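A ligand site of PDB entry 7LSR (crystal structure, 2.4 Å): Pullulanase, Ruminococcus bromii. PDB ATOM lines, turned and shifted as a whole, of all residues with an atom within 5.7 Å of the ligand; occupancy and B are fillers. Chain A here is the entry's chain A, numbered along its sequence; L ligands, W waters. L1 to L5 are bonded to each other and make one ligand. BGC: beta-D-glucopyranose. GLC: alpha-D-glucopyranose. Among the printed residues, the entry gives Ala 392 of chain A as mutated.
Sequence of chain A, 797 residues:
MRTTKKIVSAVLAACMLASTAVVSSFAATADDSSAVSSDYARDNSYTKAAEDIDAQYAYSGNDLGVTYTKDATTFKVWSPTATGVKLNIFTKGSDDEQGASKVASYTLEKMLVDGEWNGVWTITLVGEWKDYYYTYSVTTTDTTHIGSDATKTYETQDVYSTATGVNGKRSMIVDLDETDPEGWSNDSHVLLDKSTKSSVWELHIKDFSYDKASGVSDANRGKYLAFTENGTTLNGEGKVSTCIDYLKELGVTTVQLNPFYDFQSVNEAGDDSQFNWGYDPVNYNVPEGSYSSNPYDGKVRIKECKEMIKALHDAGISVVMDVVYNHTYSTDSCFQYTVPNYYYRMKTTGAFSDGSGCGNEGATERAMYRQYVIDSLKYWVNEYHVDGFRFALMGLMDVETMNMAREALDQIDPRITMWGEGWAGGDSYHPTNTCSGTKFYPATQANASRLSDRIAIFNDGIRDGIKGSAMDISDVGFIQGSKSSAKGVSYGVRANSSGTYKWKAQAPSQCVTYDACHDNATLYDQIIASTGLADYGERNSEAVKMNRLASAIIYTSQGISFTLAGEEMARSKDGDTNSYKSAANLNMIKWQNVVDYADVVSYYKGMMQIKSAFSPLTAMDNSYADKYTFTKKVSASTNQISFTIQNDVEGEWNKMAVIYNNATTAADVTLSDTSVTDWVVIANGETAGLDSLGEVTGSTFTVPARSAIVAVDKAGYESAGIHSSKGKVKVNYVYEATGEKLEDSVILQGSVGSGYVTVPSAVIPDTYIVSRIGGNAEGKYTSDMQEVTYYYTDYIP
The guanidinium group of Arg 390 lies within hydrogen-bond range of an oxygen (O2) of BGC L1 (2.9 Å).
O2 of GLC L2 is in hydrogen-bond range of OD1 of Asn 578 (2.6 Å).
ND2 of Asn 360 sits at hydrogen-bond distance from O2 of GLC L5 (3.3 Å).
A ring nitrogen (NE2) of His 518 sits at hydrogen-bond distance from an oxygen (O3) of BGC L1 (2.8 Å).
O2 of GLC L5 lies within hydrogen-bond range of O of Cys 358, 3.4 Å away.
An oxygen (O3) of GLC L5 sits at hydrogen-bond distance from the side-chain hydroxyl (OG1) of Thr 331 (3.0 Å).
The side-chain carboxylate (OE2) of Glu 421 sits at hydrogen-bond distance from an oxygen (O1) of BGC L1, at 2.6 Å.
The side-chain carboxylate (OD2) of Asp 519 is in hydrogen-bond range of an oxygen (O2) of BGC L1 (2.5 Å).
OD1 of Asp 280 sits at hydrogen-bond distance from O6 of GLC L2 (2.7 Å).
N of Thr 331 is in hydrogen-bond range of O3 of GLC L5, at 2.8 Å.
The side-chain hydroxyl (OH) of Tyr 279 sits at hydrogen-bond distance from the side-chain carboxylate (OD2) of Asp 322 (2.6 Å).
A ring nitrogen (NE2) of His 327 lies within hydrogen-bond range of the backbone carbonyl oxygen (O) of Tyr 279, 3.2 Å away.
The side-chain amide nitrogen of Asn 326 sits at hydrogen-bond distance from the backbone carbonyl oxygen of Ala 392, at 2.9 Å.
The backbone NH of Cys 358 lies within hydrogen-bond range of the side-chain carboxylate of Asp 354 (3.1 Å).
The backbone NH of Gly 357 sits at hydrogen-bond distance from the side-chain carboxylate of Asp 354.
The backbone NH (N) of Leu 393 lies within hydrogen-bond range of the side-chain carboxylate (OE2) of Glu 421 (3.0 Å).
A ring nitrogen (NE2) of His 518 lies within hydrogen-bond range of the side-chain carboxylate (OD2) of Asp 519, 3.2 Å away.
NH2 of Arg 390 lies within salt-bridge range of OE1 of Glu 421 (3.5 Å).
CZ3 of Trp 277 touches O3 of BGC L1, at 3.4 Å.
Tyr 279 touches the ligand.
CE1 of His 327 touches O6 of BGC L1 (3.9 Å).
O of Tyr 329 touches O2 of GLC L5, 3.6 Å away.
CA of Ser 330 touches O3 of GLC L5 (3.3 Å).
O of Ser 356 touches O6 of BGC L1, 3.8 Å away.
O of Gly 357 touches O2 of GLC L4 (3.8 Å).
CA of Gly 359 touches O2 of GLC L5 (3.5 Å).
CB of Ala 392 touches O1 of BGC L1, 3.1 Å away.
CD1 of Leu 393 touches O6 of BGC L1 (3.3 Å).
Tyr 580 touches the ligand.
Hydrophobic or aromatic side chains that line the ligand: Trp 277, Tyr 279, His 327, Tyr 329, Ala 392, Leu 393, His 518 and Tyr 580.
Water W3 lies within hydrogen-bond range of O6 of BGC L1 (2.6 Å) and ND2 of Asn 326 (2.8 Å).
Water W1 lies within hydrogen-bond range of the side-chain amide oxygen (OD1) of Asn 276 (2.7 Å), an oxygen (O6) of GLC L2 (2.7 Å), the backbone NH (N) of Tyr 279 (2.7 Å) and the backbone NH (N) of Gly 278 (3.1 Å).
Water W2 lies within hydrogen-bond range of OD2 of Asp 280, O6 of GLC L2 and ND2 of Asn 276.
Water W4 lies within hydrogen-bond range of the side-chain carboxylate of Asp 354 (2.7 Å), an oxygen (O3) of GLC L4 (2.8 Å), the backbone carbonyl oxygen of Gly 357 (2.9 Å) and the backbone NH of Gly 359 (3.3 Å).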
ATOM      1  N   ASN A 276      27.188  -4.253 -29.212  1.00  0.00           N
ATOM      2  CA  ASN A 276      26.099  -4.065 -28.274  1.00  0.00           C
ATOM      3  C   ASN A 276      24.929  -3.368 -28.990  1.00  0.00           C
ATOM      4  O   ASN A 276      25.142  -2.497 -29.831  1.00  0.00           O
ATOM      5  CB  ASN A 276      26.535  -3.277 -27.023  1.00  0.00           C
ATOM      6  CG  ASN A 276      25.631  -3.515 -25.840  1.00  0.00           C
ATOM      7  OD1 ASN A 276      24.512  -3.003 -25.791  1.00  0.00           O
ATOM      8  ND2 ASN A 276      26.095  -4.289 -24.872  1.00  0.00           N
ATOM      9  N   TRP A 277      23.704  -3.778 -28.638  1.00  0.00           N
ATOM     10  CA  TRP A 277      22.486  -3.111 -29.102  1.00  0.00           C
ATOM     11  C   TRP A 277      22.526  -1.630 -28.707  1.00  0.00           C
ATOM     12  O   TRP A 277      22.125  -0.760 -29.481  1.00  0.00           O
ATOM     13  CB  TRP A 277      21.225  -3.796 -28.550  1.00  0.00           C
ATOM     14  CG  TRP A 277      20.929  -5.155 -29.104  1.00  0.00           C
ATOM     15  CD1 TRP A 277      21.369  -5.701 -30.273  1.00  0.00           C
ATOM     16  CD2 TRP A 277      20.056  -6.132 -28.509  1.00  0.00           C
ATOM     17  NE1 TRP A 277      20.858  -6.955 -30.438  1.00  0.00           N
ATOM     18  CE2 TRP A 277      20.054  -7.254 -29.369  1.00  0.00           C
ATOM     19  CE3 TRP A 277      19.309  -6.190 -27.327  1.00  0.00           C
ATOM     20  CZ2 TRP A 277      19.317  -8.408 -29.089  1.00  0.00           C
ATOM     21  CZ3 TRP A 277      18.585  -7.325 -27.048  1.00  0.00           C
ATOM     22  CH2 TRP A 277      18.581  -8.416 -27.921  1.00  0.00           C
ATOM     23  N   GLY A 278      22.998  -1.376 -27.483  1.00  0.00           N
ATOM     24  CA  GLY A 278      23.270  -0.032 -26.978  1.00  0.00           C
ATOM     25  C   GLY A 278      22.073   0.566 -26.258  1.00  0.00           C
ATOM     26  O   GLY A 278      21.795   1.758 -26.399  1.00  0.00           O
ATOM     27  N   TYR A 279      21.384  -0.263 -25.453  1.00  0.00           N
ATOM     28  CA  TYR A 279      20.285   0.189 -24.582  1.00  0.00           C
ATOM     29  C   TYR A 279      20.866   0.628 -23.240  1.00  0.00           C
ATOM     30  O   TYR A 279      20.386   0.226 -22.179  1.00  0.00           O
ATOM     31  CB  TYR A 279      19.220  -0.909 -24.459  1.00  0.00           C
ATOM     32  CG  TYR A 279      18.474  -1.177 -25.742  1.00  0.00           C
ATOM     33  CD1 TYR A 279      17.446  -0.345 -26.152  1.00  0.00           C
ATOM     34  CD2 TYR A 279      18.804  -2.244 -26.557  1.00  0.00           C
ATOM     35  CE1 TYR A 279      16.763  -0.565 -27.336  1.00  0.00           C
ATOM     36  CE2 TYR A 279      18.124  -2.485 -27.739  1.00  0.00           C
ATOM     37  CZ  TYR A 279      17.102  -1.642 -28.130  1.00  0.00           C
ATOM     38  OH  TYR A 279      16.434  -1.871 -29.301  1.00  0.00           O
ATOM     39  N   ASP A 280      21.896   1.480 -23.308  1.00  0.00           N
ATOM     40  CA  ASP A 280      22.736   1.879 -22.179  1.00  0.00           C
ATOM     41  C   ASP A 280      23.087   3.364 -22.324  1.00  0.00           C
ATOM     42  O   ASP A 280      24.260   3.706 -22.470  1.00  0.00           O
ATOM     43  CB  ASP A 280      23.997   1.015 -22.112  1.00  0.00           C
ATOM     44  CG  ASP A 280      23.722  -0.481 -22.128  1.00  0.00           C
ATOM     45  OD1 ASP A 280      22.955  -0.952 -21.273  1.00  0.00           O
ATOM     46  OD2 ASP A 280      24.280  -1.167 -23.007  1.00  0.00           O
ATOM     47  N   ASP A 322      15.155   4.445 -32.409  1.00  0.00           N
ATOM     48  CA  ASP A 322      14.929   3.771 -31.130  1.00  0.00           C
ATOM     49  C   ASP A 322      15.482   4.650 -30.013  1.00  0.00           C
ATOM     50  O   ASP A 322      16.689   4.935 -29.983  1.00  0.00           O
ATOM     51  CB  ASP A 322      15.573   2.379 -31.138  1.00  0.00           C
ATOM     52  CG  ASP A 322      15.131   1.468 -30.006  1.00  0.00           C
ATOM     53  OD1 ASP A 322      14.658   1.988 -28.976  1.00  0.00           O
ATOM     54  OD2 ASP A 322      15.247   0.242 -30.172  1.00  0.00           O
ATOM     55  N   VAL A 324      15.471   5.674 -25.662  1.00  0.00           N
ATOM     56  CA  VAL A 324      15.511   4.966 -24.387  1.00  0.00           C
ATOM     57  C   VAL A 324      15.627   5.999 -23.254  1.00  0.00           C
ATOM     58  O   VAL A 324      16.586   5.998 -22.488  1.00  0.00           O
ATOM     59  CB  VAL A 324      16.670   3.957 -24.363  1.00  0.00           C
ATOM     60  CG1 VAL A 324      16.627   3.047 -23.143  1.00  0.00           C
ATOM     61  CG2 VAL A 324      16.710   3.125 -25.632  1.00  0.00           C
ATOM     62  N   ASN A 326      13.692   6.037 -20.796  1.00  0.00           N
ATOM     63  CA  ASN A 326      13.124   5.367 -19.635  1.00  0.00           C
ATOM     64  C   ASN A 326      14.192   5.140 -18.564  1.00  0.00           C
ATOM     65  O   ASN A 326      13.854   5.014 -17.393  1.00  0.00           O
ATOM     66  CB  ASN A 326      12.417   4.066 -20.018  1.00  0.00           C
ATOM     67  CG  ASN A 326      13.376   2.940 -20.351  1.00  0.00           C
ATOM     68  OD1 ASN A 326      13.932   2.309 -19.458  1.00  0.00           O
ATOM     69  ND2 ASN A 326      13.544   2.656 -21.634  1.00  0.00           N
ATOM     70  N   HIS A 327      15.477   5.072 -18.959  1.00  0.00           N
ATOM     71  CA  HIS A 327      16.585   4.869 -18.012  1.00  0.00           C
ATOM     72  C   HIS A 327      17.920   5.306 -18.642  1.00  0.00           C
ATOM     73  O   HIS A 327      18.024   5.434 -19.860  1.00  0.00           O
ATOM     74  CB  HIS A 327      16.652   3.403 -17.559  1.00  0.00           C
ATOM     75  CG  HIS A 327      17.324   2.496 -18.533  1.00  0.00           C
ATOM     76  ND1 HIS A 327      16.709   2.085 -19.703  1.00  0.00           N
ATOM     77  CD2 HIS A 327      18.541   1.920 -18.522  1.00  0.00           C
ATOM     78  CE1 HIS A 327      17.526   1.291 -20.368  1.00  0.00           C
ATOM     79  NE2 HIS A 327      18.664   1.183 -19.673  1.00  0.00           N
ATOM     80  N   THR A 328      18.917   5.514 -17.781  1.00  0.00           N
ATOM     81  CA  THR A 328      20.320   5.701 -18.182  1.00  0.00           C
ATOM     82  C   THR A 328      21.123   4.486 -17.692  1.00  0.00           C
ATOM     83  O   THR A 328      20.679   3.751 -16.812  1.00  0.00           O
ATOM     84  CB  THR A 328      20.898   7.009 -17.633  1.00  0.00           C
ATOM     85  OG1 THR A 328      20.855   6.968 -16.208  1.00  0.00           O
ATOM     86  CG2 THR A 328      20.161   8.233 -18.131  1.00  0.00           C
ATOM     87  N   TYR A 329      22.318   4.301 -18.266  1.00  0.00           N
ATOM     88  CA  TYR A 329      23.165   3.140 -17.975  1.00  0.00           C
ATOM     89  C   TYR A 329      23.453   3.058 -16.471  1.00  0.00           C
ATOM     90  O   TYR A 329      23.318   1.991 -15.862  1.00  0.00           O
ATOM     91  CB  TYR A 329      24.474   3.183 -18.761  1.00  0.00           C
ATOM     92  CG  TYR A 329      25.463   2.112 -18.355  1.00  0.00           C
ATOM     93  CD1 TYR A 329      25.192   0.775 -18.590  1.00  0.00           C
ATOM     94  CD2 TYR A 329      26.640   2.434 -17.705  1.00  0.00           C
ATOM     95  CE1 TYR A 329      26.086  -0.214 -18.212  1.00  0.00           C
ATOM     96  CE2 TYR A 329      27.540   1.451 -17.321  1.00  0.00           C
ATOM     97  CZ  TYR A 329      27.258   0.116 -17.566  1.00  0.00           C
ATOM     98  OH  TYR A 329      28.143  -0.857 -17.195  1.00  0.00           O
ATOM     99  N   SER A 330      23.872   4.183 -15.895  1.00  0.00           N
ATOM    100  CA  SER A 330      24.138   4.295 -14.457  1.00  0.00           C
ATOM    101  C   SER A 330      23.595   5.624 -13.931  1.00  0.00           C
ATOM    102  O   SER A 330      23.328   6.547 -14.704  1.00  0.00           O
ATOM    103  CB  SER A 330      25.616   4.161 -14.170  1.00  0.00           C
ATOM    104  OG  SER A 330      26.306   5.362 -14.452  1.00  0.00           O
ATOM    105  N   THR A 331      23.439   5.696 -12.605  1.00  0.00           N
ATOM    106  CA  THR A 331      23.032   6.918 -11.920  1.00  0.00           C
ATOM    107  C   THR A 331      24.224   7.864 -11.786  1.00  0.00           C
ATOM    108  O   THR A 331      24.050   9.016 -11.419  1.00  0.00           O
ATOM    109  CB  THR A 331      22.380   6.585 -10.567  1.00  0.00           C
ATOM    110  OG1 THR A 331      23.279   5.770  -9.816  1.00  0.00           O
ATOM    111  CG2 THR A 331      21.055   5.879 -10.718  1.00  0.00           C
ATOM    112  N   ASP A 332      25.434   7.369 -12.062  1.00  0.00           N
ATOM    113  CA  ASP A 332      26.610   8.212 -12.295  1.00  0.00           C
ATOM    114  C   ASP A 332      26.509   8.791 -13.709  1.00  0.00           C
ATOM    115  O   ASP A 332      27.260   8.398 -14.608  1.00  0.00           O
ATOM    116  CB  ASP A 332      27.915   7.436 -12.079  1.00  0.00           C
ATOM    117  CG  ASP A 332      28.200   7.074 -10.626  1.00  0.00           C
ATOM    118  OD1 ASP A 332      27.600   7.705  -9.732  1.00  0.00           O
ATOM    119  OD2 ASP A 332      29.020   6.165 -10.405  1.00  0.00           O
ATOM    120  N   ASP A 354      13.558   0.665  -9.839  1.00  0.00           N
ATOM    121  CA  ASP A 354      14.153  -0.187 -10.867  1.00  0.00           C
ATOM    122  C   ASP A 354      13.044  -0.791 -11.734  1.00  0.00           C
ATOM    123  O   ASP A 354      12.876  -2.011 -11.805  1.00  0.00           O
ATOM    124  CB  ASP A 354      15.040  -1.252 -10.228  1.00  0.00           C
ATOM    125  CG  ASP A 354      15.980  -1.960 -11.196  1.00  0.00           C
ATOM    126  OD1 ASP A 354      16.055  -1.521 -12.363  1.00  0.00           O
ATOM    127  OD2 ASP A 354      16.632  -2.934 -10.779  1.00  0.00           O
ATOM    128  N   SER A 356      12.914  -0.361 -15.020  1.00  0.00           N
ATOM    129  CA  SER A 356      13.553  -0.743 -16.274  1.00  0.00           C
ATOM    130  C   SER A 356      14.193  -2.135 -16.150  1.00  0.00           C
ATOM    131  O   SER A 356      14.320  -2.845 -17.149  1.00  0.00           O
ATOM    132  CB  SER A 356      14.574   0.282 -16.694  1.00  0.00           C
ATOM    133  OG  SER A 356      15.660   0.319 -15.773  1.00  0.00           O
ATOM    134  N   GLY A 357      14.598  -2.489 -14.926  1.00  0.00           N
ATOM    135  CA  GLY A 357      15.412  -3.673 -14.667  1.00  0.00           C
ATOM    136  C   GLY A 357      16.882  -3.419 -14.938  1.00  0.00           C
ATOM    137  O   GLY A 357      17.678  -4.353 -14.942  1.00  0.00           O
ATOM    138  N   CYS A 358      17.239  -2.147 -15.166  1.00  0.00           N
ATOM    139  CA  CYS A 358      18.598  -1.728 -15.505  1.00  0.00           C
ATOM    140  C   CYS A 358      19.165  -0.772 -14.453  1.00  0.00           C
ATOM    141  O   CYS A 358      20.228  -0.185 -14.663  1.00  0.00           O
ATOM    142  CB  CYS A 358      18.629  -1.084 -16.893  1.00  0.00           C
ATOM    143  SG  CYS A 358      18.229  -2.223 -18.231  1.00  0.00           S
ATOM    144  N   GLY A 359      18.450  -0.612 -13.330  1.00  0.00           N
ATOM    145  CA  GLY A 359      18.993   0.016 -12.123  1.00  0.00           C
ATOM    146  C   GLY A 359      18.336   1.351 -11.779  1.00  0.00           C
ATOM    147  O   GLY A 359      18.503   1.840 -10.659  1.00  0.00           O
ATOM    148  N   ASN A 360      17.609   1.939 -12.734  1.00  0.00           N
ATOM    149  CA  ASN A 360      16.991   3.259 -12.544  1.00  0.00           C
ATOM    150  C   ASN A 360      15.834   3.429 -13.548  1.00  0.00           C
ATOM    151  O   ASN A 360      15.629   2.581 -14.406  1.00  0.00           O
ATOM    152  CB  ASN A 360      18.011   4.386 -12.706  1.00  0.00           C
ATOM    153  CG  ASN A 360      18.690   4.382 -14.059  1.00  0.00           C
ATOM    154  OD1 ASN A 360      18.285   5.123 -14.961  1.00  0.00           O
ATOM    155  ND2 ASN A 360      19.706   3.562 -14.224  1.00  0.00           N
ATOM    156  N   ARG A 390      10.709   4.937 -31.878  1.00  0.00           N
ATOM    157  CA  ARG A 390      10.331   3.727 -31.143  1.00  0.00           C
ATOM    158  C   ARG A 390      10.781   3.893 -29.686  1.00  0.00           C
ATOM    159  O   ARG A 390      11.978   3.873 -29.393  1.00  0.00           O
ATOM    160  CB  ARG A 390      10.953   2.489 -31.783  1.00  0.00           C
ATOM    161  CG  ARG A 390      10.654   1.181 -31.061  1.00  0.00           C
ATOM    162  CD  ARG A 390      11.778   0.737 -30.136  1.00  0.00           C
ATOM    163  NE  ARG A 390      11.578  -0.603 -29.595  1.00  0.00           N
ATOM    164  CZ  ARG A 390      12.247  -1.114 -28.570  1.00  0.00           C
ATOM    165  NH1 ARG A 390      13.177  -0.398 -27.952  1.00  0.00           N
ATOM    166  NH2 ARG A 390      11.989  -2.350 -28.157  1.00  0.00           N
ATOM    167  N   PHE A 391       9.811   4.074 -28.776  1.00  0.00           N
ATOM    168  CA  PHE A 391      10.076   4.338 -27.361  1.00  0.00           C
ATOM    169  C   PHE A 391      10.287   3.015 -26.612  1.00  0.00           C
ATOM    170  O   PHE A 391       9.365   2.200 -26.499  1.00  0.00           O
ATOM    171  CB  PHE A 391       8.921   5.136 -26.744  1.00  0.00           C
ATOM    172  CG  PHE A 391       8.771   6.526 -27.301  1.00  0.00           C
ATOM    173  CD1 PHE A 391       7.989   6.758 -28.425  1.00  0.00           C
ATOM    174  CD2 PHE A 391       9.417   7.603 -26.712  1.00  0.00           C
ATOM    175  CE1 PHE A 391       7.854   8.036 -28.945  1.00  0.00           C
ATOM    176  CE2 PHE A 391       9.283   8.882 -27.232  1.00  0.00           C
ATOM    177  CZ  PHE A 391       8.497   9.091 -28.346  1.00  0.00           C
ATOM    178  N   ALA A 392      11.502   2.822 -26.107  1.00  0.00           N
ATOM    179  CA  ALA A 392      11.848   1.691 -25.258  1.00  0.00           C
ATOM    180  C   ALA A 392      11.135   1.841 -23.903  1.00  0.00           C
ATOM    181  O   ALA A 392      11.167   2.915 -23.300  1.00  0.00           O
ATOM    182  CB  ALA A 392      13.348   1.609 -25.071  1.00  0.00           C
ATOM    183  N   LEU A 393      10.501   0.745 -23.448  1.00  0.00           N
ATOM    184  CA  LEU A 393       9.714   0.699 -22.220  1.00  0.00           C
ATOM    185  C   LEU A 393       8.900   1.983 -22.073  1.00  0.00           C
ATOM    186  O   LEU A 393       9.096   2.766 -21.132  1.00  0.00           O
ATOM    187  CB  LEU A 393      10.641   0.477 -21.020  1.00  0.00           C
ATOM    188  CG  LEU A 393      11.438  -0.827 -21.035  1.00  0.00           C
ATOM    189  CD1 LEU A 393      12.299  -0.949 -19.784  1.00  0.00           C
ATOM    190  CD2 LEU A 393      10.537  -2.045 -21.172  1.00  0.00           C
ATOM    191  N   GLU A 421       6.954   0.026 -26.586  1.00  0.00           N
ATOM    192  CA  GLU A 421       6.566  -1.101 -25.749  1.00  0.00           C
ATOM    193  C   GLU A 421       5.599  -0.618 -24.665  1.00  0.00           C
ATOM    194  O   GLU A 421       5.969   0.214 -23.835  1.00  0.00           O
ATOM    195  CB  GLU A 421       7.787  -1.720 -25.065  1.00  0.00           C
ATOM    196  CG  GLU A 421       8.751  -2.409 -26.024  1.00  0.00           C
ATOM    197  CD  GLU A 421      10.068  -2.790 -25.380  1.00  0.00           C
ATOM    198  OE1 GLU A 421      10.448  -3.973 -25.470  1.00  0.00           O
ATOM    199  OE2 GLU A 421      10.714  -1.899 -24.784  1.00  0.00           O
ATOM    200  N   HIS A 518      14.134  -7.617 -32.379  1.00  0.00           N
ATOM    201  CA  HIS A 518      15.525  -7.877 -31.987  1.00  0.00           C
ATOM    202  C   HIS A 518      15.582  -8.729 -30.716  1.00  0.00           C
ATOM    203  O   HIS A 518      16.456  -9.584 -30.578  1.00  0.00           O
ATOM    204  CB  HIS A 518      16.300  -6.564 -31.838  1.00  0.00           C
ATOM    205  CG  HIS A 518      15.935  -5.772 -30.620  1.00  0.00           C
ATOM    206  ND1 HIS A 518      14.947  -4.813 -30.641  1.00  0.00           N
ATOM    207  CD2 HIS A 518      16.419  -5.800 -29.368  1.00  0.00           C
ATOM    208  CE1 HIS A 518      14.833  -4.283 -29.435  1.00  0.00           C
ATOM    209  NE2 HIS A 518      15.730  -4.874 -28.638  1.00  0.00           N
ATOM    210  N   ASP A 519      14.639  -8.488 -29.792  1.00  0.00           N
ATOM    211  CA  ASP A 519      14.573  -9.209 -28.519  1.00  0.00           C
ATOM    212  C   ASP A 519      14.124 -10.659 -28.770  1.00  0.00           C
ATOM    213  O   ASP A 519      13.466 -10.950 -29.772  1.00  0.00           O
ATOM    214  CB  ASP A 519      13.599  -8.543 -27.542  1.00  0.00           C
ATOM    215  CG  ASP A 519      14.152  -7.278 -26.897  1.00  0.00           C
ATOM    216  OD1 ASP A 519      15.277  -7.333 -26.359  1.00  0.00           O
ATOM    217  OD2 ASP A 519      13.441  -6.246 -26.948  1.00  0.00           O
ATOM    218  N   ASN A 578      18.838 -13.559 -26.428  1.00  0.00           N
ATOM    219  CA  ASN A 578      19.166 -12.246 -25.875  1.00  0.00           C
ATOM    220  C   ASN A 578      20.585 -11.870 -26.323  1.00  0.00           C
ATOM    221  O   ASN A 578      21.526 -11.921 -25.534  1.00  0.00           O
ATOM    222  CB  ASN A 578      19.001 -12.222 -24.356  1.00  0.00           C
ATOM    223  CG  ASN A 578      19.138 -10.834 -23.756  1.00  0.00           C
ATOM    224  OD1 ASN A 578      18.759  -9.847 -24.371  1.00  0.00           O
ATOM    225  ND2 ASN A 578      19.688 -10.757 -22.547  1.00  0.00           N
ATOM    226  N   TYR A 580      22.372  -9.325 -26.984  1.00  0.00           N
ATOM    227  CA  TYR A 580      22.588  -7.893 -26.796  1.00  0.00           C
ATOM    228  C   TYR A 580      24.090  -7.573 -26.769  1.00  0.00           C
ATOM    229  O   TYR A 580      24.483  -6.514 -27.239  1.00  0.00           O
ATOM    230  CB  TYR A 580      21.861  -7.389 -25.550  1.00  0.00           C
ATOM    231  CG  TYR A 580      22.475  -7.743 -24.218  1.00  0.00           C
ATOM    232  CD1 TYR A 580      22.197  -8.949 -23.595  1.00  0.00           C
ATOM    233  CD2 TYR A 580      23.319  -6.859 -23.566  1.00  0.00           C
ATOM    234  CE1 TYR A 580      22.743  -9.280 -22.364  1.00  0.00           C
ATOM    235  CE2 TYR A 580      23.872  -7.170 -22.328  1.00  0.00           C
ATOM    236  CZ  TYR A 580      23.590  -8.380 -21.735  1.00  0.00           C
ATOM    237  OH  TYR A 580      24.121  -8.701 -20.518  1.00  0.00           O
HETATM  238  C2  BGC L   1      14.722  -3.321 -25.498  1.00  0.00           C
HETATM  239  C3  BGC L   1      15.542  -4.450 -24.881  1.00  0.00           C
HETATM  240  C4  BGC L   1      16.373  -3.912 -23.715  1.00  0.00           C
HETATM  241  C5  BGC L   1      15.455  -3.195 -22.727  1.00  0.00           C
HETATM  242  C6  BGC L   1      16.212  -2.655 -21.519  1.00  0.00           C
HETATM  243  C1  BGC L   1      13.920  -2.585 -24.432  1.00  0.00           C
HETATM  244  O1  BGC L   1      13.242  -1.482 -25.042  1.00  0.00           O
HETATM  245  O2  BGC L   1      13.839  -3.843 -26.496  1.00  0.00           O
HETATM  246  O3  BGC L   1      16.378  -5.016 -25.898  1.00  0.00           O
HETATM  247  O4  BGC L   1      17.052  -4.980 -23.035  1.00  0.00           O
HETATM  248  O5  BGC L   1      14.782  -2.121 -23.401  1.00  0.00           O
HETATM  249  O6  BGC L   1      15.354  -1.874 -20.703  1.00  0.00           O
HETATM  250  C1  GLC L   2      18.374  -5.194 -23.564  1.00  0.00           C
HETATM  251  C2  GLC L   2      18.850  -6.586 -23.170  1.00  0.00           C
HETATM  252  C3  GLC L   2      19.193  -6.657 -21.683  1.00  0.00           C
HETATM  253  C4  GLC L   2      20.159  -5.539 -21.316  1.00  0.00           C
HETATM  254  C5  GLC L   2      19.601  -4.187 -21.743  1.00  0.00           C
HETATM  255  C6  GLC L   2      20.553  -3.046 -21.442  1.00  0.00           C
HETATM  256  O2  GLC L   2      17.828  -7.542 -23.475  1.00  0.00           O
HETATM  257  O3  GLC L   2      19.760  -7.940 -21.380  1.00  0.00           O
HETATM  258  O4  GLC L   2      20.373  -5.564 -19.888  1.00  0.00           O
HETATM  259  O5  GLC L   2      19.316  -4.201 -23.141  1.00  0.00           O
HETATM  260  O6  GLC L   2      21.667  -3.054 -22.351  1.00  0.00           O
HETATM  261  C1  GLC L   3      21.649  -6.137 -19.557  1.00  0.00           C
HETATM  262  C2  GLC L   3      21.525  -6.982 -18.286  1.00  0.00           C
HETATM  263  C3  GLC L   3      21.349  -6.099 -17.057  1.00  0.00           C
HETATM  264  C4  GLC L   3      22.458  -5.060 -16.995  1.00  0.00           C
HETATM  265  C5  GLC L   3      22.470  -4.260 -18.300  1.00  0.00           C
HETATM  266  C6  GLC L   3      23.541  -3.173 -18.324  1.00  0.00           C
HETATM  267  O2  GLC L   3      20.412  -7.872 -18.400  1.00  0.00           O
HETATM  268  O3  GLC L   3      21.361  -6.909 -15.878  1.00  0.00           O
HETATM  269  O4  GLC L   3      22.242  -4.169 -15.881  1.00  0.00           O
HETATM  270  O5  GLC L   3      22.674  -5.157 -19.411  1.00  0.00           O
HETATM  271  O6  GLC L   3      24.844  -3.753 -18.142  1.00  0.00           O
HETATM  272  C1  GLC L   4      23.133  -4.444 -14.769  1.00  0.00           C
HETATM  273  C2  GLC L   4      22.362  -4.336 -13.455  1.00  0.00           C
HETATM  274  C3  GLC L   4      22.015  -2.888 -13.125  1.00  0.00           C
HETATM  275  C4  GLC L   4      23.270  -2.022 -13.153  1.00  0.00           C
HETATM  276  C5  GLC L   4      23.931  -2.186 -14.527  1.00  0.00           C
HETATM  277  C6  GLC L   4      25.192  -1.343 -14.685  1.00  0.00           C
HETATM  278  O2  GLC L   4      21.163  -5.109 -13.535  1.00  0.00           O
HETATM  279  O3  GLC L   4      21.391  -2.868 -11.830  1.00  0.00           O
HETATM  280  O4  GLC L   4      22.987  -0.615 -12.956  1.00  0.00           O
HETATM  281  O5  GLC L   4      24.254  -3.566 -14.742  1.00  0.00           O
HETATM  282  O6  GLC L   4      26.188  -1.771 -13.753  1.00  0.00           O
HETATM  283  C1  GLC L   5      22.759  -0.229 -11.575  1.00  0.00           C
HETATM  284  C2  GLC L   5      22.730   1.295 -11.469  1.00  0.00           C
HETATM  285  C3  GLC L   5      24.127   1.903 -11.525  1.00  0.00           C
HETATM  286  C4  GLC L   5      25.013   1.262 -10.457  1.00  0.00           C
HETATM  287  C5  GLC L   5      25.019  -0.250 -10.664  1.00  0.00           C
HETATM  288  C6  GLC L   5      25.852  -0.938  -9.578  1.00  0.00           C
HETATM  289  O2  GLC L   5      21.941   1.842 -12.534  1.00  0.00           O
HETATM  290  O3  GLC L   5      24.052   3.319 -11.303  1.00  0.00           O
HETATM  291  O4  GLC L   5      26.335   1.792 -10.530  1.00  0.00           O
HETATM  292  O5  GLC L   5      23.690  -0.775 -10.625  1.00  0.00           O
HETATM  293  O6  GLC L   5      25.665  -2.356  -9.646  1.00  0.00           O
HETATM  294  O   HOH W   1      21.902  -2.921 -25.065  1.00  0.00           O
HETATM  295  O   HOH W   2      24.387  -3.727 -22.287  1.00  0.00           O
HETATM  296  O   HOH W   3      14.877   0.280 -22.159  1.00  0.00           O
HETATM  297  O   HOH W   4      18.741  -3.743 -12.275  1.00  0.00           O
